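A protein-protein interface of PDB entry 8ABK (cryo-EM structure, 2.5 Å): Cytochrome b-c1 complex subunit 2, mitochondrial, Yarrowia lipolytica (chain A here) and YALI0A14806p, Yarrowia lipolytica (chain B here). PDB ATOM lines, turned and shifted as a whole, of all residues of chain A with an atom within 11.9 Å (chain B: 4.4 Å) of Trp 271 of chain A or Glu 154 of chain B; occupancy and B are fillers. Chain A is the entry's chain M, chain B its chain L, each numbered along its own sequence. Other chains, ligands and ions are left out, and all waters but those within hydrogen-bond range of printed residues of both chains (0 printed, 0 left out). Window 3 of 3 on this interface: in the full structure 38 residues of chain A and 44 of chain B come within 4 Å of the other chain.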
ATOM      1  N   GLY A 265      22.600  -0.685   7.232  1.00  0.00           N
ATOM      2  CA  GLY A 265      21.839   0.527   6.998  1.00  0.00           C
ATOM      3  C   GLY A 265      22.609   1.561   6.178  1.00  0.00           C
ATOM      4  O   GLY A 265      22.083   2.037   5.171  1.00  0.00           O
ATOM      5  N   PRO A 266      23.817   1.994   6.617  1.00  0.00           N
ATOM      6  CA  PRO A 266      24.640   2.903   5.817  1.00  0.00           C
ATOM      7  C   PRO A 266      25.289   2.170   4.644  1.00  0.00           C
ATOM      8  O   PRO A 266      25.453   0.949   4.684  1.00  0.00           O
ATOM      9  CB  PRO A 266      25.681   3.446   6.806  1.00  0.00           C
ATOM     10  CG  PRO A 266      25.772   2.394   7.902  1.00  0.00           C
ATOM     11  CD  PRO A 266      24.448   1.660   7.905  1.00  0.00           C
ATOM     12  N   ALA A 267      25.604   2.928   3.586  1.00  0.00           N
ATOM     13  CA  ALA A 267      26.160   2.374   2.358  1.00  0.00           C
ATOM     14  C   ALA A 267      27.675   2.239   2.483  1.00  0.00           C
ATOM     15  O   ALA A 267      28.324   3.026   3.170  1.00  0.00           O
ATOM     16  CB  ALA A 267      25.768   3.218   1.168  1.00  0.00           C
ATOM     17  N   SER A 268      28.226   1.240   1.797  1.00  0.00           N
ATOM     18  CA  SER A 268      29.639   0.949   1.926  1.00  0.00           C
ATOM     19  C   SER A 268      30.400   1.499   0.725  1.00  0.00           C
ATOM     20  O   SER A 268      31.592   1.225   0.579  1.00  0.00           O
ATOM     21  CB  SER A 268      29.857  -0.521   2.138  1.00  0.00           C
ATOM     22  OG  SER A 268      29.188  -1.283   1.145  1.00  0.00           O
ATOM     23  N   MET A 269      29.701   2.298  -0.094  1.00  0.00           N
ATOM     24  CA  MET A 269      30.284   2.897  -1.277  1.00  0.00           C
ATOM     25  C   MET A 269      29.480   4.136  -1.670  1.00  0.00           C
ATOM     26  O   MET A 269      28.293   4.239  -1.376  1.00  0.00           O
ATOM     27  CB  MET A 269      30.444   1.884  -2.421  1.00  0.00           C
ATOM     28  CG  MET A 269      29.207   1.629  -3.202  1.00  0.00           C
ATOM     29  SD  MET A 269      29.529   0.279  -4.339  1.00  0.00           S
ATOM     30  CE  MET A 269      28.154   0.456  -5.470  1.00  0.00           C
ATOM     31  N   PRO A 270      30.121   5.163  -2.263  1.00  0.00           N
ATOM     32  CA  PRO A 270      29.449   6.438  -2.522  1.00  0.00           C
ATOM     33  C   PRO A 270      28.327   6.304  -3.545  1.00  0.00           C
ATOM     34  O   PRO A 270      28.380   5.452  -4.425  1.00  0.00           O
ATOM     35  CB  PRO A 270      30.570   7.315  -3.090  1.00  0.00           C
ATOM     36  CG  PRO A 270      31.839   6.662  -2.624  1.00  0.00           C
ATOM     37  CD  PRO A 270      31.531   5.185  -2.682  1.00  0.00           C
ATOM     38  N   TRP A 271      27.299   7.146  -3.386  1.00  0.00           N
ATOM     39  CA  TRP A 271      26.193   7.269  -4.328  1.00  0.00           C
ATOM     40  C   TRP A 271      25.447   5.950  -4.501  1.00  0.00           C
ATOM     41  O   TRP A 271      24.880   5.701  -5.556  1.00  0.00           O
ATOM     42  CB  TRP A 271      26.693   7.776  -5.684  1.00  0.00           C
ATOM     43  CG  TRP A 271      27.773   8.802  -5.571  1.00  0.00           C
ATOM     44  CD1 TRP A 271      29.075   8.681  -5.962  1.00  0.00           C
ATOM     45  CD2 TRP A 271      27.644  10.106  -4.987  1.00  0.00           C
ATOM     46  NE1 TRP A 271      29.757   9.838  -5.701  1.00  0.00           N
ATOM     47  CE2 TRP A 271      28.911  10.724  -5.088  1.00  0.00           C
ATOM     48  CE3 TRP A 271      26.585  10.808  -4.396  1.00  0.00           C
ATOM     49  CZ2 TRP A 271      29.142  12.017  -4.619  1.00  0.00           C
ATOM     50  CZ3 TRP A 271      26.815  12.086  -3.935  1.00  0.00           C
ATOM     51  CH2 TRP A 271      28.077  12.678  -4.044  1.00  0.00           C
ATOM     52  N   SER A 272      25.467   5.098  -3.480  1.00  0.00           N
ATOM     53  CA  SER A 272      24.805   3.813  -3.585  1.00  0.00           C
ATOM     54  C   SER A 272      23.848   3.660  -2.414  1.00  0.00           C
ATOM     55  O   SER A 272      23.865   4.473  -1.495  1.00  0.00           O
ATOM     56  CB  SER A 272      25.808   2.701  -3.629  1.00  0.00           C
ATOM     57  OG  SER A 272      25.933   2.060  -2.371  1.00  0.00           O
ATOM     58  N   VAL A 273      23.039   2.602  -2.457  1.00  0.00           N
ATOM     59  CA  VAL A 273      22.093   2.355  -1.385  1.00  0.00           C
ATOM     60  C   VAL A 273      22.704   1.355  -0.406  1.00  0.00           C
ATOM     61  O   VAL A 273      22.698   1.588   0.799  1.00  0.00           O
ATOM     62  CB  VAL A 273      20.693   1.969  -1.914  1.00  0.00           C
ATOM     63  CG1 VAL A 273      20.033   0.871  -1.105  1.00  0.00           C
ATOM     64  CG2 VAL A 273      19.778   3.179  -2.009  1.00  0.00           C
ATOM     65  N   GLY A 274      23.255   0.259  -0.936  1.00  0.00           N
ATOM     66  CA  GLY A 274      23.863  -0.766  -0.104  1.00  0.00           C
ATOM     67  C   GLY A 274      23.085  -2.076  -0.175  1.00  0.00           C
ATOM     68  O   GLY A 274      21.934  -2.098  -0.594  1.00  0.00           O
ATOM     69  N   ALA A 275      23.720  -3.169   0.262  1.00  0.00           N
ATOM     70  CA  ALA A 275      23.190  -4.508   0.059  1.00  0.00           C
ATOM     71  C   ALA A 275      22.600  -5.055   1.355  1.00  0.00           C
ATOM     72  O   ALA A 275      22.153  -6.203   1.400  1.00  0.00           O
ATOM     73  CB  ALA A 275      24.286  -5.398  -0.465  1.00  0.00           C
ATOM     74  N   ALA A 279      19.293  -1.106   4.414  1.00  0.00           N
ATOM     75  CA  ALA A 279      19.674  -0.147   3.388  1.00  0.00           C
ATOM     76  C   ALA A 279      18.670  -0.224   2.245  1.00  0.00           C
ATOM     77  O   ALA A 279      18.250   0.804   1.720  1.00  0.00           O
ATOM     78  CB  ALA A 279      21.077  -0.410   2.895  1.00  0.00           C
ATOM     79  N   GLN A 280      18.276  -1.464   1.918  1.00  0.00           N
ATOM     80  CA  GLN A 280      17.366  -1.791   0.831  1.00  0.00           C
ATOM     81  C   GLN A 280      15.929  -1.381   1.168  1.00  0.00           C
ATOM     82  O   GLN A 280      15.045  -1.424   0.316  1.00  0.00           O
ATOM     83  CB  GLN A 280      17.464  -3.288   0.516  1.00  0.00           C
ATOM     84  CG  GLN A 280      18.641  -3.657  -0.383  1.00  0.00           C
ATOM     85  CD  GLN A 280      18.531  -3.103  -1.787  1.00  0.00           C
ATOM     86  OE1 GLN A 280      17.456  -3.069  -2.383  1.00  0.00           O
ATOM     87  NE2 GLN A 280      19.648  -2.644  -2.326  1.00  0.00           N
ATOM     88  N   THR A 282      15.227   1.541   2.190  1.00  0.00           N
ATOM     89  CA  THR A 282      15.130   2.968   1.949  1.00  0.00           C
ATOM     90  C   THR A 282      14.913   3.284   0.475  1.00  0.00           C
ATOM     91  O   THR A 282      14.807   4.461   0.147  1.00  0.00           O
ATOM     92  CB  THR A 282      16.390   3.712   2.394  1.00  0.00           C
ATOM     93  OG1 THR A 282      17.468   3.221   1.598  1.00  0.00           O
ATOM     94  CG2 THR A 282      16.702   3.510   3.857  1.00  0.00           C
ATOM     95  N   VAL A 283      14.813   2.262  -0.388  1.00  0.00           N
ATOM     96  CA  VAL A 283      14.864   2.522  -1.822  1.00  0.00           C
ATOM     97  C   VAL A 283      13.594   3.247  -2.261  1.00  0.00           C
ATOM     98  O   VAL A 283      12.487   2.827  -1.935  1.00  0.00           O
ATOM     99  CB  VAL A 283      15.181   1.276  -2.678  1.00  0.00           C
ATOM    100  CG1 VAL A 283      16.578   0.738  -2.396  1.00  0.00           C
ATOM    101  CG2 VAL A 283      14.141   0.169  -2.549  1.00  0.00           C
ATOM    102  N   GLY A 284      13.798   4.381  -2.936  1.00  0.00           N
ATOM    103  CA  GLY A 284      12.709   5.225  -3.387  1.00  0.00           C
ATOM    104  C   GLY A 284      12.463   6.386  -2.434  1.00  0.00           C
ATOM    105  O   GLY A 284      11.579   7.208  -2.668  1.00  0.00           O
ATOM    106  N   THR A 285      13.265   6.440  -1.366  1.00  0.00           N
ATOM    107  CA  THR A 285      13.136   7.471  -0.351  1.00  0.00           C
ATOM    108  C   THR A 285      14.488   8.133  -0.097  1.00  0.00           C
ATOM    109  O   THR A 285      15.534   7.488  -0.204  1.00  0.00           O
ATOM    110  CB  THR A 285      12.550   6.906   0.953  1.00  0.00           C
ATOM    111  OG1 THR A 285      13.407   5.870   1.415  1.00  0.00           O
ATOM    112  CG2 THR A 285      11.160   6.329   0.802  1.00  0.00           C
ATOM    113  N   HIS A 286      14.440   9.416   0.282  1.00  0.00           N
ATOM    114  CA  HIS A 286      15.609  10.143   0.755  1.00  0.00           C
ATOM    115  C   HIS A 286      15.715   9.991   2.271  1.00  0.00           C
ATOM    116  O   HIS A 286      15.599  10.959   3.021  1.00  0.00           O
ATOM    117  CB  HIS A 286      15.573  11.608   0.293  1.00  0.00           C
ATOM    118  CG  HIS A 286      15.312  11.760  -1.166  1.00  0.00           C
ATOM    119  ND1 HIS A 286      16.142  11.209  -2.121  1.00  0.00           N
ATOM    120  CD2 HIS A 286      14.315  12.379  -1.833  1.00  0.00           C
ATOM    121  CE1 HIS A 286      15.670  11.487  -3.319  1.00  0.00           C
ATOM    122  NE2 HIS A 286      14.549  12.206  -3.170  1.00  0.00           N
ATOM    123  N   THR A 287      15.902   8.750   2.722  1.00  0.00           N
ATOM    124  CA  THR A 287      15.998   8.457   4.139  1.00  0.00           C
ATOM    125  C   THR A 287      17.250   7.625   4.367  1.00  0.00           C
ATOM    126  O   THR A 287      17.725   6.934   3.469  1.00  0.00           O
ATOM    127  CB  THR A 287      14.775   7.685   4.651  1.00  0.00           C
ATOM    128  OG1 THR A 287      14.616   6.575   3.769  1.00  0.00           O
ATOM    129  CG2 THR A 287      13.488   8.480   4.673  1.00  0.00           C
ATOM    130  N   HIS B  74      33.128  14.930 -11.917  1.00  0.00           N
ATOM    131  CA  HIS B  74      32.272  14.611 -10.797  1.00  0.00           C
ATOM    132  C   HIS B  74      31.215  13.599 -11.227  1.00  0.00           C
ATOM    133  O   HIS B  74      30.789  12.777 -10.418  1.00  0.00           O
ATOM    134  CB  HIS B  74      31.680  15.890 -10.221  1.00  0.00           C
ATOM    135  CG  HIS B  74      30.635  15.659  -9.181  1.00  0.00           C
ATOM    136  ND1 HIS B  74      30.937  15.227  -7.904  1.00  0.00           N
ATOM    137  CD2 HIS B  74      29.288  15.734  -9.245  1.00  0.00           C
ATOM    138  CE1 HIS B  74      29.820  15.071  -7.222  1.00  0.00           C
ATOM    139  NE2 HIS B  74      28.793  15.398  -8.013  1.00  0.00           N
ATOM    140  N   GLU B  77      32.702  10.093 -11.070  1.00  0.00           N
ATOM    141  CA  GLU B  77      32.759   9.605  -9.703  1.00  0.00           C
ATOM    142  C   GLU B  77      31.455   8.893  -9.322  1.00  0.00           C
ATOM    143  O   GLU B  77      31.482   7.981  -8.500  1.00  0.00           O
ATOM    144  CB  GLU B  77      33.076  10.774  -8.767  1.00  0.00           C
ATOM    145  CG  GLU B  77      33.230  10.362  -7.316  1.00  0.00           C
ATOM    146  CD  GLU B  77      33.122  11.460  -6.275  1.00  0.00           C
ATOM    147  OE1 GLU B  77      33.435  12.614  -6.600  1.00  0.00           O
ATOM    148  OE2 GLU B  77      32.773  11.137  -5.116  1.00  0.00           O
ATOM    149  N   HIS B  78      30.313   9.362  -9.845  1.00  0.00           N
ATOM    150  CA  HIS B  78      29.019   8.757  -9.582  1.00  0.00           C
ATOM    151  C   HIS B  78      28.808   7.474 -10.367  1.00  0.00           C
ATOM    152  O   HIS B  78      27.823   6.791 -10.096  1.00  0.00           O
ATOM    153  CB  HIS B  78      27.876   9.654 -10.060  1.00  0.00           C
ATOM    154  CG  HIS B  78      27.549  10.760  -9.126  1.00  0.00           C
ATOM    155  ND1 HIS B  78      26.369  10.800  -8.415  1.00  0.00           N
ATOM    156  CD2 HIS B  78      28.236  11.880  -8.813  1.00  0.00           C
ATOM    157  CE1 HIS B  78      26.344  11.900  -7.695  1.00  0.00           C
ATOM    158  NE2 HIS B  78      27.478  12.576  -7.922  1.00  0.00           N
ATOM    159  N   PHE B  81      30.760   3.783  -9.559  1.00  0.00           N
ATOM    160  CA  PHE B  81      30.144   2.863  -8.619  1.00  0.00           C
ATOM    161  C   PHE B  81      28.885   2.219  -9.186  1.00  0.00           C
ATOM    162  O   PHE B  81      28.212   1.481  -8.478  1.00  0.00           O
ATOM    163  CB  PHE B  81      29.974   3.513  -7.246  1.00  0.00           C
ATOM    164  CG  PHE B  81      31.291   3.947  -6.659  1.00  0.00           C
ATOM    165  CD1 PHE B  81      32.155   3.016  -6.105  1.00  0.00           C
ATOM    166  CD2 PHE B  81      31.700   5.271  -6.735  1.00  0.00           C
ATOM    167  CE1 PHE B  81      33.376   3.407  -5.575  1.00  0.00           C
ATOM    168  CE2 PHE B  81      32.924   5.662  -6.217  1.00  0.00           C
ATOM    169  CZ  PHE B  81      33.756   4.730  -5.633  1.00  0.00           C
ATOM    170  N   LYS B  82      28.653   2.402 -10.489  1.00  0.00           N
ATOM    171  CA  LYS B  82      27.396   1.976 -11.081  1.00  0.00           C
ATOM    172  C   LYS B  82      27.577   0.733 -11.953  1.00  0.00           C
ATOM    173  O   LYS B  82      26.688   0.394 -12.734  1.00  0.00           O
ATOM    174  CB  LYS B  82      26.737   3.103 -11.882  1.00  0.00           C
ATOM    175  CG  LYS B  82      26.266   4.313 -11.092  1.00  0.00           C
ATOM    176  CD  LYS B  82      25.015   4.178 -10.248  1.00  0.00           C
ATOM    177  CE  LYS B  82      25.088   4.997  -8.974  1.00  0.00           C
ATOM    178  NZ  LYS B  82      25.497   4.202  -7.794  1.00  0.00           N
ATOM    179  N   VAL B 150      19.990  12.642 -10.343  1.00  0.00           N
ATOM    180  CA  VAL B 150      20.568  12.619  -9.009  1.00  0.00           C
ATOM    181  C   VAL B 150      21.492  13.821  -8.828  1.00  0.00           C
ATOM    182  O   VAL B 150      21.481  14.471  -7.782  1.00  0.00           O
ATOM    183  CB  VAL B 150      21.339  11.306  -8.791  1.00  0.00           C
ATOM    184  CG1 VAL B 150      21.994  11.240  -7.420  1.00  0.00           C
ATOM    185  CG2 VAL B 150      20.447  10.103  -9.021  1.00  0.00           C
ATOM    186  N   ILE B 151      22.305  14.071  -9.857  1.00  0.00           N
ATOM    187  CA  ILE B 151      23.260  15.161  -9.858  1.00  0.00           C
ATOM    188  C   ILE B 151      22.504  16.478 -10.002  1.00  0.00           C
ATOM    189  O   ILE B 151      22.926  17.483  -9.434  1.00  0.00           O
ATOM    190  CB  ILE B 151      24.321  14.947 -10.955  1.00  0.00           C
ATOM    191  CG1 ILE B 151      25.271  13.805 -10.589  1.00  0.00           C
ATOM    192  CG2 ILE B 151      25.080  16.231 -11.255  1.00  0.00           C
ATOM    193  CD1 ILE B 151      26.071  13.288 -11.762  1.00  0.00           C
ATOM    194  N   THR B 152      21.397  16.465 -10.756  1.00  0.00           N
ATOM    195  CA  THR B 152      20.598  17.671 -10.911  1.00  0.00           C
ATOM    196  C   THR B 152      20.020  18.097  -9.562  1.00  0.00           C
ATOM    197  O   THR B 152      19.989  19.286  -9.268  1.00  0.00           O
ATOM    198  CB  THR B 152      19.577  17.553 -12.049  1.00  0.00           C
ATOM    199  OG1 THR B 152      20.315  17.661 -13.264  1.00  0.00           O
ATOM    200  CG2 THR B 152      18.483  18.596 -12.008  1.00  0.00           C
ATOM    201  N   ARG B 153      19.618  17.121  -8.735  1.00  0.00           N
ATOM    202  CA  ARG B 153      19.100  17.382  -7.399  1.00  0.00           C
ATOM    203  C   ARG B 153      20.191  17.868  -6.442  1.00  0.00           C
ATOM    204  O   ARG B 153      19.873  18.480  -5.422  1.00  0.00           O
ATOM    205  CB  ARG B 153      18.429  16.134  -6.818  1.00  0.00           C
ATOM    206  CG  ARG B 153      17.260  16.465  -5.901  1.00  0.00           C
ATOM    207  CD  ARG B 153      16.716  15.347  -5.030  1.00  0.00           C
ATOM    208  NE  ARG B 153      17.530  15.070  -3.851  1.00  0.00           N
ATOM    209  CZ  ARG B 153      18.361  14.038  -3.719  1.00  0.00           C
ATOM    210  NH1 ARG B 153      18.506  13.160  -4.699  1.00  0.00           N
ATOM    211  NH2 ARG B 153      19.047  13.885  -2.599  1.00  0.00           N
ATOM    212  N   GLU B 154      21.458  17.552  -6.738  1.00  0.00           N
ATOM    213  CA  GLU B 154      22.567  17.937  -5.881  1.00  0.00           C
ATOM    214  C   GLU B 154      22.816  19.435  -6.012  1.00  0.00           C
ATOM    215  O   GLU B 154      23.293  20.048  -5.066  1.00  0.00           O
ATOM    216  CB  GLU B 154      23.846  17.214  -6.294  1.00  0.00           C
ATOM    217  CG  GLU B 154      24.104  15.878  -5.629  1.00  0.00           C
ATOM    218  CD  GLU B 154      25.439  15.278  -6.053  1.00  0.00           C
ATOM    219  OE1 GLU B 154      25.665  15.127  -7.283  1.00  0.00           O
ATOM    220  OE2 GLU B 154      26.266  14.984  -5.163  1.00  0.00           O
ATOM    221  N   LEU B 155      22.530  19.993  -7.198  1.00  0.00           N
ATOM    222  CA  LEU B 155      22.597  21.424  -7.450  1.00  0.00           C
ATOM    223  C   LEU B 155      21.720  22.215  -6.478  1.00  0.00           C
ATOM    224  O   LEU B 155      22.052  23.347  -6.143  1.00  0.00           O
ATOM    225  CB  LEU B 155      22.136  21.711  -8.879  1.00  0.00           C
ATOM    226  CG  LEU B 155      23.177  21.588  -9.984  1.00  0.00           C
ATOM    227  CD1 LEU B 155      22.500  21.843 -11.317  1.00  0.00           C
ATOM    228  CD2 LEU B 155      24.310  22.583  -9.790  1.00  0.00           C
ATOM    229  N   GLU B 156      20.591  21.641  -6.040  1.00  0.00           N
ATOM    230  CA  GLU B 156      19.659  22.396  -5.212  1.00  0.00           C
ATOM    231  C   GLU B 156      19.705  21.990  -3.741  1.00  0.00           C
ATOM    232  O   GLU B 156      18.723  22.201  -3.032  1.00  0.00           O
ATOM    233  CB  GLU B 156      18.229  22.187  -5.699  1.00  0.00           C
ATOM    234  CG  GLU B 156      18.040  22.635  -7.119  1.00  0.00           C
ATOM    235  CD  GLU B 156      17.030  21.828  -7.919  1.00  0.00           C
ATOM    236  OE1 GLU B 156      16.719  20.676  -7.535  1.00  0.00           O
ATOM    237  OE2 GLU B 156      16.544  22.362  -8.923  1.00  0.00           O
ATOM    238  N   GLU B 157      20.833  21.435  -3.271  1.00  0.00           N
ATOM    239  CA  GLU B 157      20.926  20.934  -1.906  1.00  0.00           C
ATOM    240  C   GLU B 157      22.292  21.230  -1.289  1.00  0.00           C
ATOM    241  O   GLU B 157      22.451  21.083  -0.076  1.00  0.00           O
ATOM    242  CB  GLU B 157      20.599  19.443  -1.840  1.00  0.00           C
ATOM    243  CG  GLU B 157      19.113  19.146  -1.735  1.00  0.00           C
ATOM    244  CD  GLU B 157      18.702  17.769  -2.236  1.00  0.00           C
ATOM    245  OE1 GLU B 157      19.554  17.084  -2.835  1.00  0.00           O
ATOM    246  OE2 GLU B 157      17.534  17.381  -2.028  1.00  0.00           O
ATOM    247  N   VAL B 158      23.273  21.601  -2.138  1.00  0.00           N
ATOM    248  CA  VAL B 158      24.532  22.204  -1.703  1.00  0.00           C
ATOM    249  C   VAL B 158      24.220  23.548  -1.055  1.00  0.00           C
ATOM    250  O   VAL B 158      24.970  23.988  -0.194  1.00  0.00           O
ATOM    251  CB  VAL B 158      25.588  22.383  -2.822  1.00  0.00           C
ATOM    252  CG1 VAL B 158      25.102  23.273  -3.958  1.00  0.00           C
ATOM    253  CG2 VAL B 158      26.900  22.930  -2.278  1.00  0.00           C
ATOM    254  N   LEU B 185      30.707  20.503  -9.704  1.00  0.00           N
ATOM    255  CA  LEU B 185      29.479  19.919 -10.219  1.00  0.00           C
ATOM    256  C   LEU B 185      29.238  20.336 -11.658  1.00  0.00           C
ATOM    257  O   LEU B 185      28.730  19.552 -12.450  1.00  0.00           O
ATOM    258  CB  LEU B 185      28.307  20.345  -9.349  1.00  0.00           C
ATOM    259  CG  LEU B 185      27.826  19.228  -8.437  1.00  0.00           C
ATOM    260  CD1 LEU B 185      28.631  19.191  -7.146  1.00  0.00           C
ATOM    261  CD2 LEU B 185      26.367  19.444  -8.164  1.00  0.00           C
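Of the 19 printed residues of chain A, 4 touch a printed residue of chain B. Among the printed residues, no Asp or Glu carboxylate lies within 4 Å of a Lys or Arg side-chain nitrogen of the other chain.
Trp 271 of chain A touches just these residues of chain B: Glu 77 (3.3 Å), His 78 (3.5 Å), Lys 82 (2.8 Å) and Glu 154 (3.1 Å). Of chain A, only Trp 271 comes within 4 Å of Glu 154 of chain B. Glu 77 of chain B touches one residue of chain A. Of the printed residues of chain A, His 78 of chain B touches Trp 271 (3.5 Å). No residue of chain A comes within 4 Å of Val 150 of chain B. Ile 151 of chain B touches none of the printed residues of chain A. No residue of chain A comes within 4 Å of Thr 152 of chain B. Of chain A, only His 286 comes within 4 Å of Arg 153 of chain B. No residue of chain A comes within 4 Å of Leu 155 of chain B. Glu 156 of chain B touches none of the printed residues of chain A. No residue of chain A comes within 4 Å of Glu 157 of chain B. No residue of chain A comes within 4 Å of Leu 185 of chain B. Of the printed residues of chain A, Lys 82 of chain B touches Trp 271 (2.8 Å). Of the printed residues of chain B, Met 269 of chain A touches Phe 81. Printed residues of chain B within 4 Å of Pro 270 of chain A: Phe 81. Printed residues of chain B within 4 Å of His 286 of chain A: Arg 153 (3.6 Å). Thr 285 of chain A touches none of the printed residues of chain B.
The indole nitrogen (NE1) of Trp 271 of chain A is in hydrogen-bond range of the side-chain carboxylate (OE2) of Glu 77 of chain B, at 3.3 Å. The backbone carbonyl oxygen (O) of Trp 271 of chain A is in hydrogen-bond range of the side-chain amino group (NZ) of Lys 82 of chain B (2.8 Å).
NE2 of His 74 of chain B lies within hydrogen-bond range of NE2 of His 78 of chain B, 3.1 Å away. The side-chain carboxylate (OE1) of Glu 154 of chain B lies within hydrogen-bond range of a ring nitrogen (NE2) of His 74 of chain B (3.2 Å). A ring nitrogen (NE2) of His 78 of chain B sits at hydrogen-bond distance from the side-chain carboxylate (OE1) of Glu 154 of chain B (3.2 Å). The guanidinium group (NE) of Arg 153 of chain B lies within salt-bridge range of the side-chain carboxylate (OE2) of Glu 157 of chain B (2.9 Å). The side-chain hydroxyl (OG) of Ser 272 of chain A sits at hydrogen-bond distance from the backbone carbonyl oxygen (O) of Met 269 of chain A.
Phe 81 of chain B touches Met 269 of chain A. Phe 81 of chain B touches Pro 270 of chain A (CZ to CD, 3.7 Å). Trp 271 of chain A touches His 78 of chain B. Glu 154 of chain B touches Trp 271 of chain A. Arg 153 of chain B touches His 286 of chain A.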
